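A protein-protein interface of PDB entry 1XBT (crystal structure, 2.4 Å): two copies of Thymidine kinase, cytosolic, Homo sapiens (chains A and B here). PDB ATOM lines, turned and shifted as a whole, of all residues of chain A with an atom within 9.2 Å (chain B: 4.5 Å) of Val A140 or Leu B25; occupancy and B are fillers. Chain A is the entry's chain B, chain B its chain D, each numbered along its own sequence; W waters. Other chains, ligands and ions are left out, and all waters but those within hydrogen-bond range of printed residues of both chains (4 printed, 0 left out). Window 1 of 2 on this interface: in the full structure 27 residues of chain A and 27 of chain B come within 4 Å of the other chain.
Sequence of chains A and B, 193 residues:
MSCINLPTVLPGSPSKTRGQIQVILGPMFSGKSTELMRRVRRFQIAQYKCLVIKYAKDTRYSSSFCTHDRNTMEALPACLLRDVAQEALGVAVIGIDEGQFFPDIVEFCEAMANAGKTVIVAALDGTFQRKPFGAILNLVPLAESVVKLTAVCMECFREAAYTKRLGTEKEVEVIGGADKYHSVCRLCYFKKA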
ATOM      1  N   ILE A  21       3.137  -8.397  19.432  1.00  0.00           N
ATOM      2  CA  ILE A  21       2.811  -7.142  20.119  1.00  0.00           C
ATOM      3  C   ILE A  21       4.069  -6.297  20.271  1.00  0.00           C
ATOM      4  O   ILE A  21       5.071  -6.748  20.827  1.00  0.00           O
ATOM      5  CB  ILE A  21       2.167  -7.382  21.518  1.00  0.00           C
ATOM      6  CG1 ILE A  21       0.866  -8.186  21.407  1.00  0.00           C
ATOM      7  CG2 ILE A  21       1.934  -6.041  22.263  1.00  0.00           C
ATOM      8  CD1 ILE A  21       0.349  -8.685  22.730  1.00  0.00           C
ATOM      9  N   GLN A  22       4.007  -5.072  19.765  1.00  0.00           N
ATOM     10  CA  GLN A  22       5.079  -4.105  19.956  1.00  0.00           C
ATOM     11  C   GLN A  22       4.544  -2.948  20.789  1.00  0.00           C
ATOM     12  O   GLN A  22       3.433  -2.466  20.554  1.00  0.00           O
ATOM     13  CB  GLN A  22       5.587  -3.590  18.618  1.00  0.00           C
ATOM     14  CG  GLN A  22       6.025  -4.681  17.671  1.00  0.00           C
ATOM     15  CD  GLN A  22       6.422  -4.149  16.307  1.00  0.00           C
ATOM     16  OE1 GLN A  22       6.526  -2.931  16.101  1.00  0.00           O
ATOM     17  NE2 GLN A  22       6.656  -5.063  15.367  1.00  0.00           N
ATOM     18  N   VAL A  23       5.336  -2.514  21.763  1.00  0.00           N
ATOM     19  CA  VAL A  23       4.925  -1.459  22.673  1.00  0.00           C
ATOM     20  C   VAL A  23       5.912  -0.293  22.612  1.00  0.00           C
ATOM     21  O   VAL A  23       7.133  -0.488  22.734  1.00  0.00           O
ATOM     22  CB  VAL A  23       4.799  -1.984  24.123  1.00  0.00           C
ATOM     23  CG1 VAL A  23       4.292  -0.885  25.047  1.00  0.00           C
ATOM     24  CG2 VAL A  23       3.872  -3.198  24.183  1.00  0.00           C
ATOM     25  N   ILE A  24       5.366   0.901  22.376  1.00  0.00           N
ATOM     26  CA  ILE A  24       6.120   2.142  22.326  1.00  0.00           C
ATOM     27  C   ILE A  24       5.707   2.986  23.531  1.00  0.00           C
ATOM     28  O   ILE A  24       4.584   3.480  23.603  1.00  0.00           O
ATOM     29  CB  ILE A  24       5.849   2.917  20.999  1.00  0.00           C
ATOM     30  CG1 ILE A  24       6.001   2.011  19.772  1.00  0.00           C
ATOM     31  CG2 ILE A  24       6.751   4.138  20.878  1.00  0.00           C
ATOM     32  CD1 ILE A  24       5.344   2.582  18.511  1.00  0.00           C
ATOM     33  N   LEU A  25       6.626   3.120  24.477  1.00  0.00           N
ATOM     34  CA  LEU A  25       6.400   3.865  25.705  1.00  0.00           C
ATOM     35  C   LEU A  25       7.185   5.169  25.673  1.00  0.00           C
ATOM     36  O   LEU A  25       8.018   5.382  24.798  1.00  0.00           O
ATOM     37  CB  LEU A  25       6.812   3.022  26.909  1.00  0.00           C
ATOM     38  CG  LEU A  25       6.033   1.719  27.156  1.00  0.00           C
ATOM     39  CD1 LEU A  25       6.626   0.963  28.350  1.00  0.00           C
ATOM     40  CD2 LEU A  25       4.536   1.964  27.372  1.00  0.00           C
ATOM     41  N   ILE A 105      -7.025  -3.194  27.099  1.00  0.00           N
ATOM     42  CA  ILE A 105      -5.829  -3.230  26.251  1.00  0.00           C
ATOM     43  C   ILE A 105      -5.124  -4.579  26.222  1.00  0.00           C
ATOM     44  O   ILE A 105      -4.717  -5.053  25.154  1.00  0.00           O
ATOM     45  CB  ILE A 105      -4.829  -2.068  26.588  1.00  0.00           C
ATOM     46  CG1 ILE A 105      -3.652  -2.051  25.596  1.00  0.00           C
ATOM     47  CG2 ILE A 105      -4.286  -2.188  28.006  1.00  0.00           C
ATOM     48  CD1 ILE A 105      -3.898  -1.273  24.298  1.00  0.00           C
ATOM     49  N   VAL A 106      -5.008  -5.211  27.384  1.00  0.00           N
ATOM     50  CA  VAL A 106      -4.259  -6.457  27.522  1.00  0.00           C
ATOM     51  C   VAL A 106      -4.940  -7.620  26.786  1.00  0.00           C
ATOM     52  O   VAL A 106      -4.312  -8.260  25.935  1.00  0.00           O
ATOM     53  CB  VAL A 106      -3.968  -6.774  29.027  1.00  0.00           C
ATOM     54  CG1 VAL A 106      -3.323  -8.129  29.203  1.00  0.00           C
ATOM     55  CG2 VAL A 106      -3.088  -5.691  29.634  1.00  0.00           C
ATOM     56  N   CYS A 109      -5.017  -7.048  22.795  1.00  0.00           N
ATOM     57  CA  CYS A 109      -3.739  -7.212  22.102  1.00  0.00           C
ATOM     58  C   CYS A 109      -3.315  -8.667  22.073  1.00  0.00           C
ATOM     59  O   CYS A 109      -2.859  -9.175  21.043  1.00  0.00           O
ATOM     60  CB  CYS A 109      -2.648  -6.345  22.729  1.00  0.00           C
ATOM     61  SG  CYS A 109      -2.960  -4.572  22.590  1.00  0.00           S
ATOM     62  N   GLU A 110      -3.493  -9.337  23.207  1.00  0.00           N
ATOM     63  CA  GLU A 110      -3.135 -10.739  23.338  1.00  0.00           C
ATOM     64  C   GLU A 110      -3.976 -11.602  22.383  1.00  0.00           C
ATOM     65  O   GLU A 110      -3.448 -12.464  21.682  1.00  0.00           O
ATOM     66  CB  GLU A 110      -3.285 -11.156  24.805  1.00  0.00           C
ATOM     67  CG  GLU A 110      -3.054 -12.628  25.091  1.00  0.00           C
ATOM     68  CD  GLU A 110      -1.611 -13.072  24.897  1.00  0.00           C
ATOM     69  OE1 GLU A 110      -1.399 -14.301  24.871  1.00  0.00           O
ATOM     70  OE2 GLU A 110      -0.694 -12.221  24.775  1.00  0.00           O
ATOM     71  N   VAL A 121       1.408  -0.663  19.821  1.00  0.00           N
ATOM     72  CA  VAL A 121       0.749   0.155  20.837  1.00  0.00           C
ATOM     73  C   VAL A 121       1.636   1.315  21.260  1.00  0.00           C
ATOM     74  O   VAL A 121       2.760   1.108  21.697  1.00  0.00           O
ATOM     75  CB  VAL A 121       0.402  -0.681  22.103  1.00  0.00           C
ATOM     76  CG1 VAL A 121      -0.451   0.132  23.100  1.00  0.00           C
ATOM     77  CG2 VAL A 121      -0.290  -1.981  21.729  1.00  0.00           C
ATOM     78  N   LEU A 124       1.635   5.994  27.218  1.00  0.00           N
ATOM     79  CA  LEU A 124       2.339   6.559  28.328  1.00  0.00           C
ATOM     80  C   LEU A 124       2.609   5.381  29.280  1.00  0.00           C
ATOM     81  O   LEU A 124       1.702   4.585  29.559  1.00  0.00           O
ATOM     82  CB  LEU A 124       1.448   7.559  29.128  1.00  0.00           C
ATOM     83  CG  LEU A 124       1.624   9.063  28.988  1.00  0.00           C
ATOM     84  CD1 LEU A 124       2.413   9.384  27.727  1.00  0.00           C
ATOM     85  CD2 LEU A 124       0.273   9.764  28.985  1.00  0.00           C
ATOM     86  N   ASP A 125       3.830   5.261  29.776  1.00  0.00           N
ATOM     87  CA  ASP A 125       4.137   4.284  30.818  1.00  0.00           C
ATOM     88  C   ASP A 125       3.695   4.794  32.196  1.00  0.00           C
ATOM     89  O   ASP A 125       3.244   4.007  33.051  1.00  0.00           O
ATOM     90  CB  ASP A 125       5.636   3.986  30.850  1.00  0.00           C
ATOM     91  CG  ASP A 125       6.488   5.251  30.842  1.00  0.00           C
ATOM     92  OD1 ASP A 125       7.589   5.229  31.446  1.00  0.00           O
ATOM     93  OD2 ASP A 125       6.149   6.318  30.268  1.00  0.00           O
ATOM     94  N   ALA A 135      -3.541  -0.325  32.927  1.00  0.00           N
ATOM     95  CA  ALA A 135      -3.130  -1.725  32.846  1.00  0.00           C
ATOM     96  C   ALA A 135      -1.970  -1.920  31.873  1.00  0.00           C
ATOM     97  O   ALA A 135      -1.550  -3.042  31.606  1.00  0.00           O
ATOM     98  CB  ALA A 135      -4.326  -2.595  32.431  1.00  0.00           C
ATOM     99  N   ILE A 136      -1.441  -0.813  31.373  1.00  0.00           N
ATOM    100  CA  ILE A 136      -0.532  -0.828  30.236  1.00  0.00           C
ATOM    101  C   ILE A 136       0.760  -1.637  30.420  1.00  0.00           C
ATOM    102  O   ILE A 136       1.251  -2.254  29.475  1.00  0.00           O
ATOM    103  CB  ILE A 136      -0.258   0.638  29.743  1.00  0.00           C
ATOM    104  CG1 ILE A 136       0.179   0.635  28.278  1.00  0.00           C
ATOM    105  CG2 ILE A 136       0.751   1.376  30.634  1.00  0.00           C
ATOM    106  CD1 ILE A 136      -0.955   0.360  27.320  1.00  0.00           C
ATOM    107  N   LEU A 137       1.287  -1.662  31.640  1.00  0.00           N
ATOM    108  CA  LEU A 137       2.532  -2.376  31.913  1.00  0.00           C
ATOM    109  C   LEU A 137       2.378  -3.903  31.876  1.00  0.00           C
ATOM    110  O   LEU A 137       3.360  -4.624  31.683  1.00  0.00           O
ATOM    111  CB  LEU A 137       3.159  -1.891  33.228  1.00  0.00           C
ATOM    112  CG  LEU A 137       3.658  -0.425  33.249  1.00  0.00           C
ATOM    113  CD1 LEU A 137       4.492  -0.129  34.496  1.00  0.00           C
ATOM    114  CD2 LEU A 137       4.429  -0.017  31.985  1.00  0.00           C
ATOM    115  N   ASN A 138       1.143  -4.389  32.031  1.00  0.00           N
ATOM    116  CA  ASN A 138       0.855  -5.819  31.867  1.00  0.00           C
ATOM    117  C   ASN A 138       1.081  -6.304  30.435  1.00  0.00           C
ATOM    118  O   ASN A 138       1.118  -7.499  30.192  1.00  0.00           O
ATOM    119  CB  ASN A 138      -0.569  -6.168  32.330  1.00  0.00           C
ATOM    120  CG  ASN A 138      -0.797  -5.901  33.819  1.00  0.00           C
ATOM    121  OD1 ASN A 138      -0.106  -6.439  34.678  1.00  0.00           O
ATOM    122  ND2 ASN A 138      -1.788  -5.075  34.122  1.00  0.00           N
ATOM    123  N   LEU A 139       1.228  -5.375  29.493  1.00  0.00           N
ATOM    124  CA  LEU A 139       1.573  -5.726  28.112  1.00  0.00           C
ATOM    125  C   LEU A 139       3.028  -6.128  27.956  1.00  0.00           C
ATOM    126  O   LEU A 139       3.351  -6.916  27.080  1.00  0.00           O
ATOM    127  CB  LEU A 139       1.296  -4.568  27.154  1.00  0.00           C
ATOM    128  CG  LEU A 139      -0.077  -4.407  26.514  1.00  0.00           C
ATOM    129  CD1 LEU A 139       0.058  -3.342  25.449  1.00  0.00           C
ATOM    130  CD2 LEU A 139      -0.631  -5.712  25.930  1.00  0.00           C
ATOM    131  N   VAL A 140       3.898  -5.568  28.798  1.00  0.00           N
ATOM    132  CA  VAL A 140       5.347  -5.772  28.689  1.00  0.00           C
ATOM    133  C   VAL A 140       5.787  -7.253  28.668  1.00  0.00           C
ATOM    134  O   VAL A 140       6.528  -7.645  27.763  1.00  0.00           O
ATOM    135  CB  VAL A 140       6.126  -4.950  29.749  1.00  0.00           C
ATOM    136  CG1 VAL A 140       7.626  -5.219  29.664  1.00  0.00           C
ATOM    137  CG2 VAL A 140       5.819  -3.445  29.603  1.00  0.00           C
ATOM    138  N   PRO A 141       5.321  -8.081  29.613  1.00  0.00           N
ATOM    139  CA  PRO A 141       5.660  -9.511  29.597  1.00  0.00           C
ATOM    140  C   PRO A 141       5.003 -10.266  28.433  1.00  0.00           C
ATOM    141  O   PRO A 141       5.378 -11.410  28.165  1.00  0.00           O
ATOM    142  CB  PRO A 141       5.125 -10.028  30.947  1.00  0.00           C
ATOM    143  CG  PRO A 141       4.773  -8.810  31.746  1.00  0.00           C
ATOM    144  CD  PRO A 141       4.441  -7.746  30.751  1.00  0.00           C
ATOM    145  N   LEU A 142       4.049  -9.636  27.751  1.00  0.00           N
ATOM    146  CA  LEU A 142       3.390 -10.258  26.594  1.00  0.00           C
ATOM    147  C   LEU A 142       3.965  -9.808  25.262  1.00  0.00           C
ATOM    148  O   LEU A 142       3.644 -10.385  24.222  1.00  0.00           O
ATOM    149  CB  LEU A 142       1.878  -9.997  26.612  1.00  0.00           C
ATOM    150  CG  LEU A 142       1.128 -10.307  27.912  1.00  0.00           C
ATOM    151  CD1 LEU A 142      -0.222  -9.615  27.920  1.00  0.00           C
ATOM    152  CD2 LEU A 142       0.966 -11.808  28.137  1.00  0.00           C
ATOM    153  N   ALA A 143       4.830  -8.795  25.294  1.00  0.00           N
ATOM    154  CA  ALA A 143       5.283  -8.133  24.070  1.00  0.00           C
ATOM    155  C   ALA A 143       6.611  -8.670  23.567  1.00  0.00           C
ATOM    156  O   ALA A 143       7.496  -9.009  24.362  1.00  0.00           O
ATOM    157  CB  ALA A 143       5.364  -6.624  24.287  1.00  0.00           C
ATOM    158  N   GLU A 144       6.757  -8.741  22.244  1.00  0.00           N
ATOM    159  CA  GLU A 144       8.024  -9.183  21.669  1.00  0.00           C
ATOM    160  C   GLU A 144       8.986  -8.020  21.500  1.00  0.00           C
ATOM    161  O   GLU A 144      10.179  -8.218  21.332  1.00  0.00           O
ATOM    162  CB  GLU A 144       7.830  -9.970  20.360  1.00  0.00           C
ATOM    163  CG  GLU A 144       6.445  -9.861  19.749  1.00  0.00           C
ATOM    164  CD  GLU A 144       5.443 -10.882  20.274  1.00  0.00           C
ATOM    165  OE1 GLU A 144       5.618 -12.093  19.995  1.00  0.00           O
ATOM    166  OE2 GLU A 144       4.457 -10.464  20.935  1.00  0.00           O
ATOM    167  N   SER A 145       8.456  -6.803  21.566  1.00  0.00           N
ATOM    168  CA  SER A 145       9.244  -5.601  21.384  1.00  0.00           C
ATOM    169  C   SER A 145       8.756  -4.497  22.320  1.00  0.00           C
ATOM    170  O   SER A 145       7.564  -4.192  22.375  1.00  0.00           O
ATOM    171  CB  SER A 145       9.157  -5.146  19.929  1.00  0.00           C
ATOM    172  OG  SER A 145      10.028  -4.059  19.677  1.00  0.00           O
ATOM    173  N   VAL A 146       9.676  -3.914  23.077  1.00  0.00           N
ATOM    174  CA  VAL A 146       9.331  -2.844  24.004  1.00  0.00           C
ATOM    175  C   VAL A 146      10.408  -1.776  23.933  1.00  0.00           C
ATOM    176  O   VAL A 146      11.591  -2.066  24.090  1.00  0.00           O
ATOM    177  CB  VAL A 146       9.178  -3.350  25.464  1.00  0.00           C
ATOM    178  CG1 VAL A 146       8.779  -2.199  26.395  1.00  0.00           C
ATOM    179  CG2 VAL A 146       8.145  -4.453  25.549  1.00  0.00           C
ATOM    180  N   VAL A 147       9.983  -0.545  23.679  1.00  0.00           N
ATOM    181  CA  VAL A 147      10.880   0.601  23.612  1.00  0.00           C
ATOM    182  C   VAL A 147      10.322   1.744  24.472  1.00  0.00           C
ATOM    183  O   VAL A 147       9.100   1.885  24.613  1.00  0.00           O
ATOM    184  CB  VAL A 147      11.097   1.037  22.132  1.00  0.00           C
ATOM    185  CG1 VAL A 147       9.961   1.905  21.623  1.00  0.00           C
ATOM    186  CG2 VAL A 147      12.402   1.757  21.969  1.00  0.00           C
ATOM    187  N   LYS A 148      11.213   2.529  25.072  1.00  0.00           N
ATOM    188  CA  LYS A 148      10.815   3.743  25.772  1.00  0.00           C
ATOM    189  C   LYS A 148      11.485   4.958  25.147  1.00  0.00           C
ATOM    190  O   LYS A 148      12.708   5.093  25.185  1.00  0.00           O
ATOM    191  CB  LYS A 148      11.117   3.668  27.275  1.00  0.00           C
ATOM    192  CG  LYS A 148      10.536   4.856  28.057  1.00  0.00           C
ATOM    193  CD  LYS A 148      10.527   4.663  29.561  1.00  0.00           C
ATOM    194  CE  LYS A 148      10.528   6.039  30.251  1.00  0.00           C
ATOM    195  NZ  LYS A 148       9.943   6.045  31.612  1.00  0.00           N
ATOM    196  N   VAL B  23      16.967   0.341  33.001  1.00  0.00           N
ATOM    197  CA  VAL B  23      16.373  -0.977  33.169  1.00  0.00           C
ATOM    198  C   VAL B  23      16.615  -1.832  31.926  1.00  0.00           C
ATOM    199  O   VAL B  23      16.362  -1.398  30.790  1.00  0.00           O
ATOM    200  CB  VAL B  23      14.887  -0.871  33.520  1.00  0.00           C
ATOM    201  CG1 VAL B  23      14.249  -2.237  33.591  1.00  0.00           C
ATOM    202  CG2 VAL B  23      14.718  -0.143  34.852  1.00  0.00           C
ATOM    203  N   ILE B  24      17.149  -3.031  32.161  1.00  0.00           N
ATOM    204  CA  ILE B  24      17.398  -4.011  31.108  1.00  0.00           C
ATOM    205  C   ILE B  24      16.474  -5.198  31.323  1.00  0.00           C
ATOM    206  O   ILE B  24      16.658  -5.977  32.265  1.00  0.00           O
ATOM    207  CB  ILE B  24      18.886  -4.484  31.094  1.00  0.00           C
ATOM    208  CG1 ILE B  24      19.844  -3.287  31.096  1.00  0.00           C
ATOM    209  CG2 ILE B  24      19.162  -5.394  29.869  1.00  0.00           C
ATOM    210  CD1 ILE B  24      21.228  -3.608  31.641  1.00  0.00           C
ATOM    211  N   LEU B  25      15.483  -5.322  30.448  1.00  0.00           N
ATOM    212  CA  LEU B  25      14.506  -6.401  30.519  1.00  0.00           C
ATOM    213  C   LEU B  25      14.764  -7.430  29.430  1.00  0.00           C
ATOM    214  O   LEU B  25      15.561  -7.203  28.525  1.00  0.00           O
ATOM    215  CB  LEU B  25      13.075  -5.857  30.390  1.00  0.00           C
ATOM    216  CG  LEU B  25      12.633  -4.816  31.426  1.00  0.00           C
ATOM    217  CD1 LEU B  25      11.229  -4.322  31.120  1.00  0.00           C
ATOM    218  CD2 LEU B  25      12.718  -5.367  32.856  1.00  0.00           C
ATOM    219  N   GLY B  26      14.069  -8.559  29.522  1.00  0.00           N
ATOM    220  CA  GLY B  26      14.171  -9.614  28.527  1.00  0.00           C
ATOM    221  C   GLY B  26      13.873 -10.969  29.145  1.00  0.00           C
ATOM    222  O   GLY B  26      13.827 -11.093  30.380  1.00  0.00           O
ATOM    223  N   LYS B  32      21.002 -10.437  29.579  1.00  0.00           N
ATOM    224  CA  LYS B  32      20.765  -9.266  30.445  1.00  0.00           C
ATOM    225  C   LYS B  32      21.927  -8.961  31.406  1.00  0.00           C
ATOM    226  O   LYS B  32      22.308  -7.799  31.554  1.00  0.00           O
ATOM    227  CB  LYS B  32      19.458  -9.402  31.221  1.00  0.00           C
ATOM    228  CG  LYS B  32      18.232  -9.638  30.359  1.00  0.00           C
ATOM    229  CD  LYS B  32      16.951  -9.772  31.198  1.00  0.00           C
ATOM    230  CE  LYS B  32      17.059 -10.897  32.237  1.00  0.00           C
ATOM    231  NZ  LYS B  32      17.089 -12.247  31.592  1.00  0.00           N
ATOM    232  N   ALA B 123      16.757  -7.496  34.738  1.00  0.00           N
ATOM    233  CA  ALA B 123      15.628  -8.222  35.307  1.00  0.00           C
ATOM    234  C   ALA B 123      14.750  -8.854  34.251  1.00  0.00           C
ATOM    235  O   ALA B 123      14.615  -8.335  33.139  1.00  0.00           O
ATOM    236  CB  ALA B 123      14.799  -7.314  36.175  1.00  0.00           C
ATOM    237  N   ASP B 125      11.210  -9.415  32.863  1.00  0.00           N
ATOM    238  CA  ASP B 125       9.945  -8.682  32.918  1.00  0.00           C
ATOM    239  C   ASP B 125       8.778  -9.611  33.233  1.00  0.00           C
ATOM    240  O   ASP B 125       7.837  -9.216  33.930  1.00  0.00           O
ATOM    241  CB  ASP B 125       9.673  -7.886  31.632  1.00  0.00           C
ATOM    242  CG  ASP B 125       9.813  -8.726  30.374  1.00  0.00           C
ATOM    243  OD1 ASP B 125       8.777  -9.192  29.850  1.00  0.00           O
ATOM    244  OD2 ASP B 125      10.916  -8.978  29.841  1.00  0.00           O
ATOM    245  N   ILE B 136       8.885  -5.422  39.624  1.00  0.00           N
ATOM    246  CA  ILE B 136       9.874  -4.857  38.713  1.00  0.00           C
ATOM    247  C   ILE B 136       9.337  -3.871  37.666  1.00  0.00           C
ATOM    248  O   ILE B 136      10.041  -2.927  37.290  1.00  0.00           O
ATOM    249  CB  ILE B 136      10.768  -5.983  38.099  1.00  0.00           C
ATOM    250  CG1 ILE B 136      12.237  -5.533  38.010  1.00  0.00           C
ATOM    251  CG2 ILE B 136      10.191  -6.553  36.790  1.00  0.00           C
ATOM    252  CD1 ILE B 136      12.582  -4.658  36.796  1.00  0.00           C
ATOM    253  N   LEU B 137       8.096  -4.055  37.218  1.00  0.00           N
ATOM    254  CA  LEU B 137       7.520  -3.138  36.231  1.00  0.00           C
ATOM    255  C   LEU B 137       7.193  -1.737  36.804  1.00  0.00           C
ATOM    256  O   LEU B 137       7.072  -0.772  36.048  1.00  0.00           O
ATOM    257  CB  LEU B 137       6.328  -3.774  35.484  1.00  0.00           C
ATOM    258  CG  LEU B 137       6.604  -5.075  34.677  1.00  0.00           C
ATOM    259  CD1 LEU B 137       5.379  -5.541  33.932  1.00  0.00           C
ATOM    260  CD2 LEU B 137       7.801  -4.990  33.714  1.00  0.00           C
ATOM    261  N   VAL B 146      14.816   2.326  29.342  1.00  0.00           N
ATOM    262  CA  VAL B 146      14.243   0.989  29.426  1.00  0.00           C
ATOM    263  C   VAL B 146      14.436   0.299  28.087  1.00  0.00           C
ATOM    264  O   VAL B 146      14.065   0.848  27.055  1.00  0.00           O
ATOM    265  CB  VAL B 146      12.740   1.031  29.793  1.00  0.00           C
ATOM    266  CG1 VAL B 146      12.097  -0.343  29.626  1.00  0.00           C
ATOM    267  CG2 VAL B 146      12.551   1.550  31.201  1.00  0.00           C
ATOM    268  N   VAL B 147      15.060  -0.883  28.110  1.00  0.00           N
ATOM    269  CA  VAL B 147      15.221  -1.718  26.915  1.00  0.00           C
ATOM    270  C   VAL B 147      14.754  -3.137  27.216  1.00  0.00           C
ATOM    271  O   VAL B 147      14.823  -3.587  28.359  1.00  0.00           O
ATOM    272  CB  VAL B 147      16.691  -1.766  26.351  1.00  0.00           C
ATOM    273  CG1 VAL B 147      17.234  -0.380  26.032  1.00  0.00           C
ATOM    274  CG2 VAL B 147      17.642  -2.509  27.291  1.00  0.00           C
ATOM    275  N   LYS B 148      14.256  -3.821  26.187  1.00  0.00           N
ATOM    276  CA  LYS B 148      13.926  -5.237  26.284  1.00  0.00           C
ATOM    277  C   LYS B 148      14.766  -6.044  25.303  1.00  0.00           C
ATOM    278  O   LYS B 148      14.646  -5.891  24.081  1.00  0.00           O
ATOM    279  CB  LYS B 148      12.436  -5.513  26.060  1.00  0.00           C
ATOM    280  CG  LYS B 148      12.051  -6.926  26.493  1.00  0.00           C
ATOM    281  CD  LYS B 148      10.582  -7.248  26.308  1.00  0.00           C
ATOM    282  CE  LYS B 148      10.365  -8.755  26.401  1.00  0.00           C
ATOM    283  NZ  LYS B 148       9.017  -9.120  26.941  1.00  0.00           N
ATOM    284  N   LEU B 149      15.627  -6.892  25.849  1.00  0.00           N
ATOM    285  CA  LEU B 149      16.488  -7.731  25.038  1.00  0.00           C
ATOM    286  C   LEU B 149      15.739  -8.947  24.518  1.00  0.00           C
ATOM    287  O   LEU B 149      14.631  -9.263  24.953  1.00  0.00           O
ATOM    288  CB  LEU B 149      17.724  -8.156  25.822  1.00  0.00           C
ATOM    289  CG  LEU B 149      18.637  -7.032  26.323  1.00  0.00           C
ATOM    290  CD1 LEU B 149      19.868  -7.621  26.998  1.00  0.00           C
ATOM    291  CD2 LEU B 149      19.028  -6.080  25.182  1.00  0.00           C
HETATM  292  O   HOH W   1      12.242  -4.802  22.576  1.00  0.00           O
HETATM  293  O   HOH W   2      14.167  -2.306  23.720  1.00  0.00           O
HETATM  294  O   HOH W   3      13.964   1.751  24.816  1.00  0.00           O
HETATM  295  O   HOH W   4      14.873   3.996  26.793  1.00  0.00           O
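O of Ala A143 lies within hydrogen-bond range of NZ of Lys B148, at 3.0 Å. The backbone carbonyl oxygen (O) of Val A140 sits close to the side-chain carboxylate (OD1) of Asp B125, at 3.4 Å. The side-chain amino group (NZ) of Lys B148 is in hydrogen-bond range of the backbone carbonyl oxygen (O) of Val A140, 3.0 Å away.
The side-chain amino group (NZ) of Lys A148 lies within salt-bridge range of the side-chain carboxylate (OD1) of Asp A125. The side-chain carboxylate (OD2) of Asp B125 lies within hydrogen-bond range of the backbone NH (N) of Gly B26 (3.2 Å). OD1 of Asp B125 is in salt-bridge range of NZ of Lys B148, at 2.9 Å. The backbone carbonyl oxygen of Leu B25 lies within hydrogen-bond range of the backbone NH of Leu B149. The backbone carbonyl oxygen (O) of Val B147 is in hydrogen-bond range of the backbone NH (N) of Leu B25 (2.8 Å).
Among the printed residues, pairs that only touch across the chains: Leu A137 with Leu B137 (3.1 Å), Pro A141 with Asp B125 (3.1 Å), Val A146 with Lys B148 (3.8 Å), Lys A148 with Val B146 (3.9 Å), Pro A141 with Leu B137 (3.98 Å) and Val A140 with Leu B25 (3.99 Å).
Ile A24 touches none of the printed residues of chain B. Printed residues of chain A within 4 Å of Leu B25: Val A140. No residue of chain A comes within 4 Å of Gly B26. Of the printed residues of chain A, Asp B125 touches Val A140 and Pro A141. Of the printed residues of chain A, Leu B137 touches Leu A137 and Pro A141. Of the printed residues of chain A, Val B146 touches Lys A148. Val B147 touches none of the printed residues of chain A. Lys B148 touches just these residues of chain A: Val A140, Ala A143 and Val A146. Leu B149 touches none of the printed residues of chain A. The nearest printed residue of chain A that does not touch Leu B25 is Val A146 (5.7 Å). The nearest printed residue of chain B that does not touch Ala A143 is Asp B125 (5.6 Å).
Of the 13 printed residues of chain B, 5 touch a printed residue of chain A. Printed residues of chain B that touch a printed residue of chain A: Leu B25, Asp B125, Leu B137, Val B146 and Lys B148. Hydrophobic or aromatic side chains of chain B within 4 Å of the printed part of chain A: Leu B25, Leu B137 and Val B146. Of the 26 printed residues of chain A, 6 touch a printed residue of chain B. Hydrophobic or aromatic side chains of chain A that line the printed part of chain B: Leu A137, Val A140, Pro A141 and Val A146. Among the printed residues, no Asp or Glu carboxylate lies within 4 Å of a Lys or Arg side-chain nitrogen of the other chain.
Leu B137 touches its own counterpart, Leu A137. Val A146 touches Lys B148, and with the chains exchanged Lys A148 touches Val B146. 9 positions are printed for both chains.
Water W3 bridges O of Val B146 (2.4 Å) and N of Lys A148 (2.9 Å). Water W2 lies within hydrogen-bond range of O of Val A146 (2.6 Å) and N of Lys B148 (2.9 Å). Water W1 lies within hydrogen-bond range of N of Val A146 (2.8 Å) and O of Lys B148 (3.0 Å). Water W4 lies within hydrogen-bond range of the backbone carbonyl oxygen of Lys A148 (2.9 Å) and the backbone NH of Val B146 (3.0 Å).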
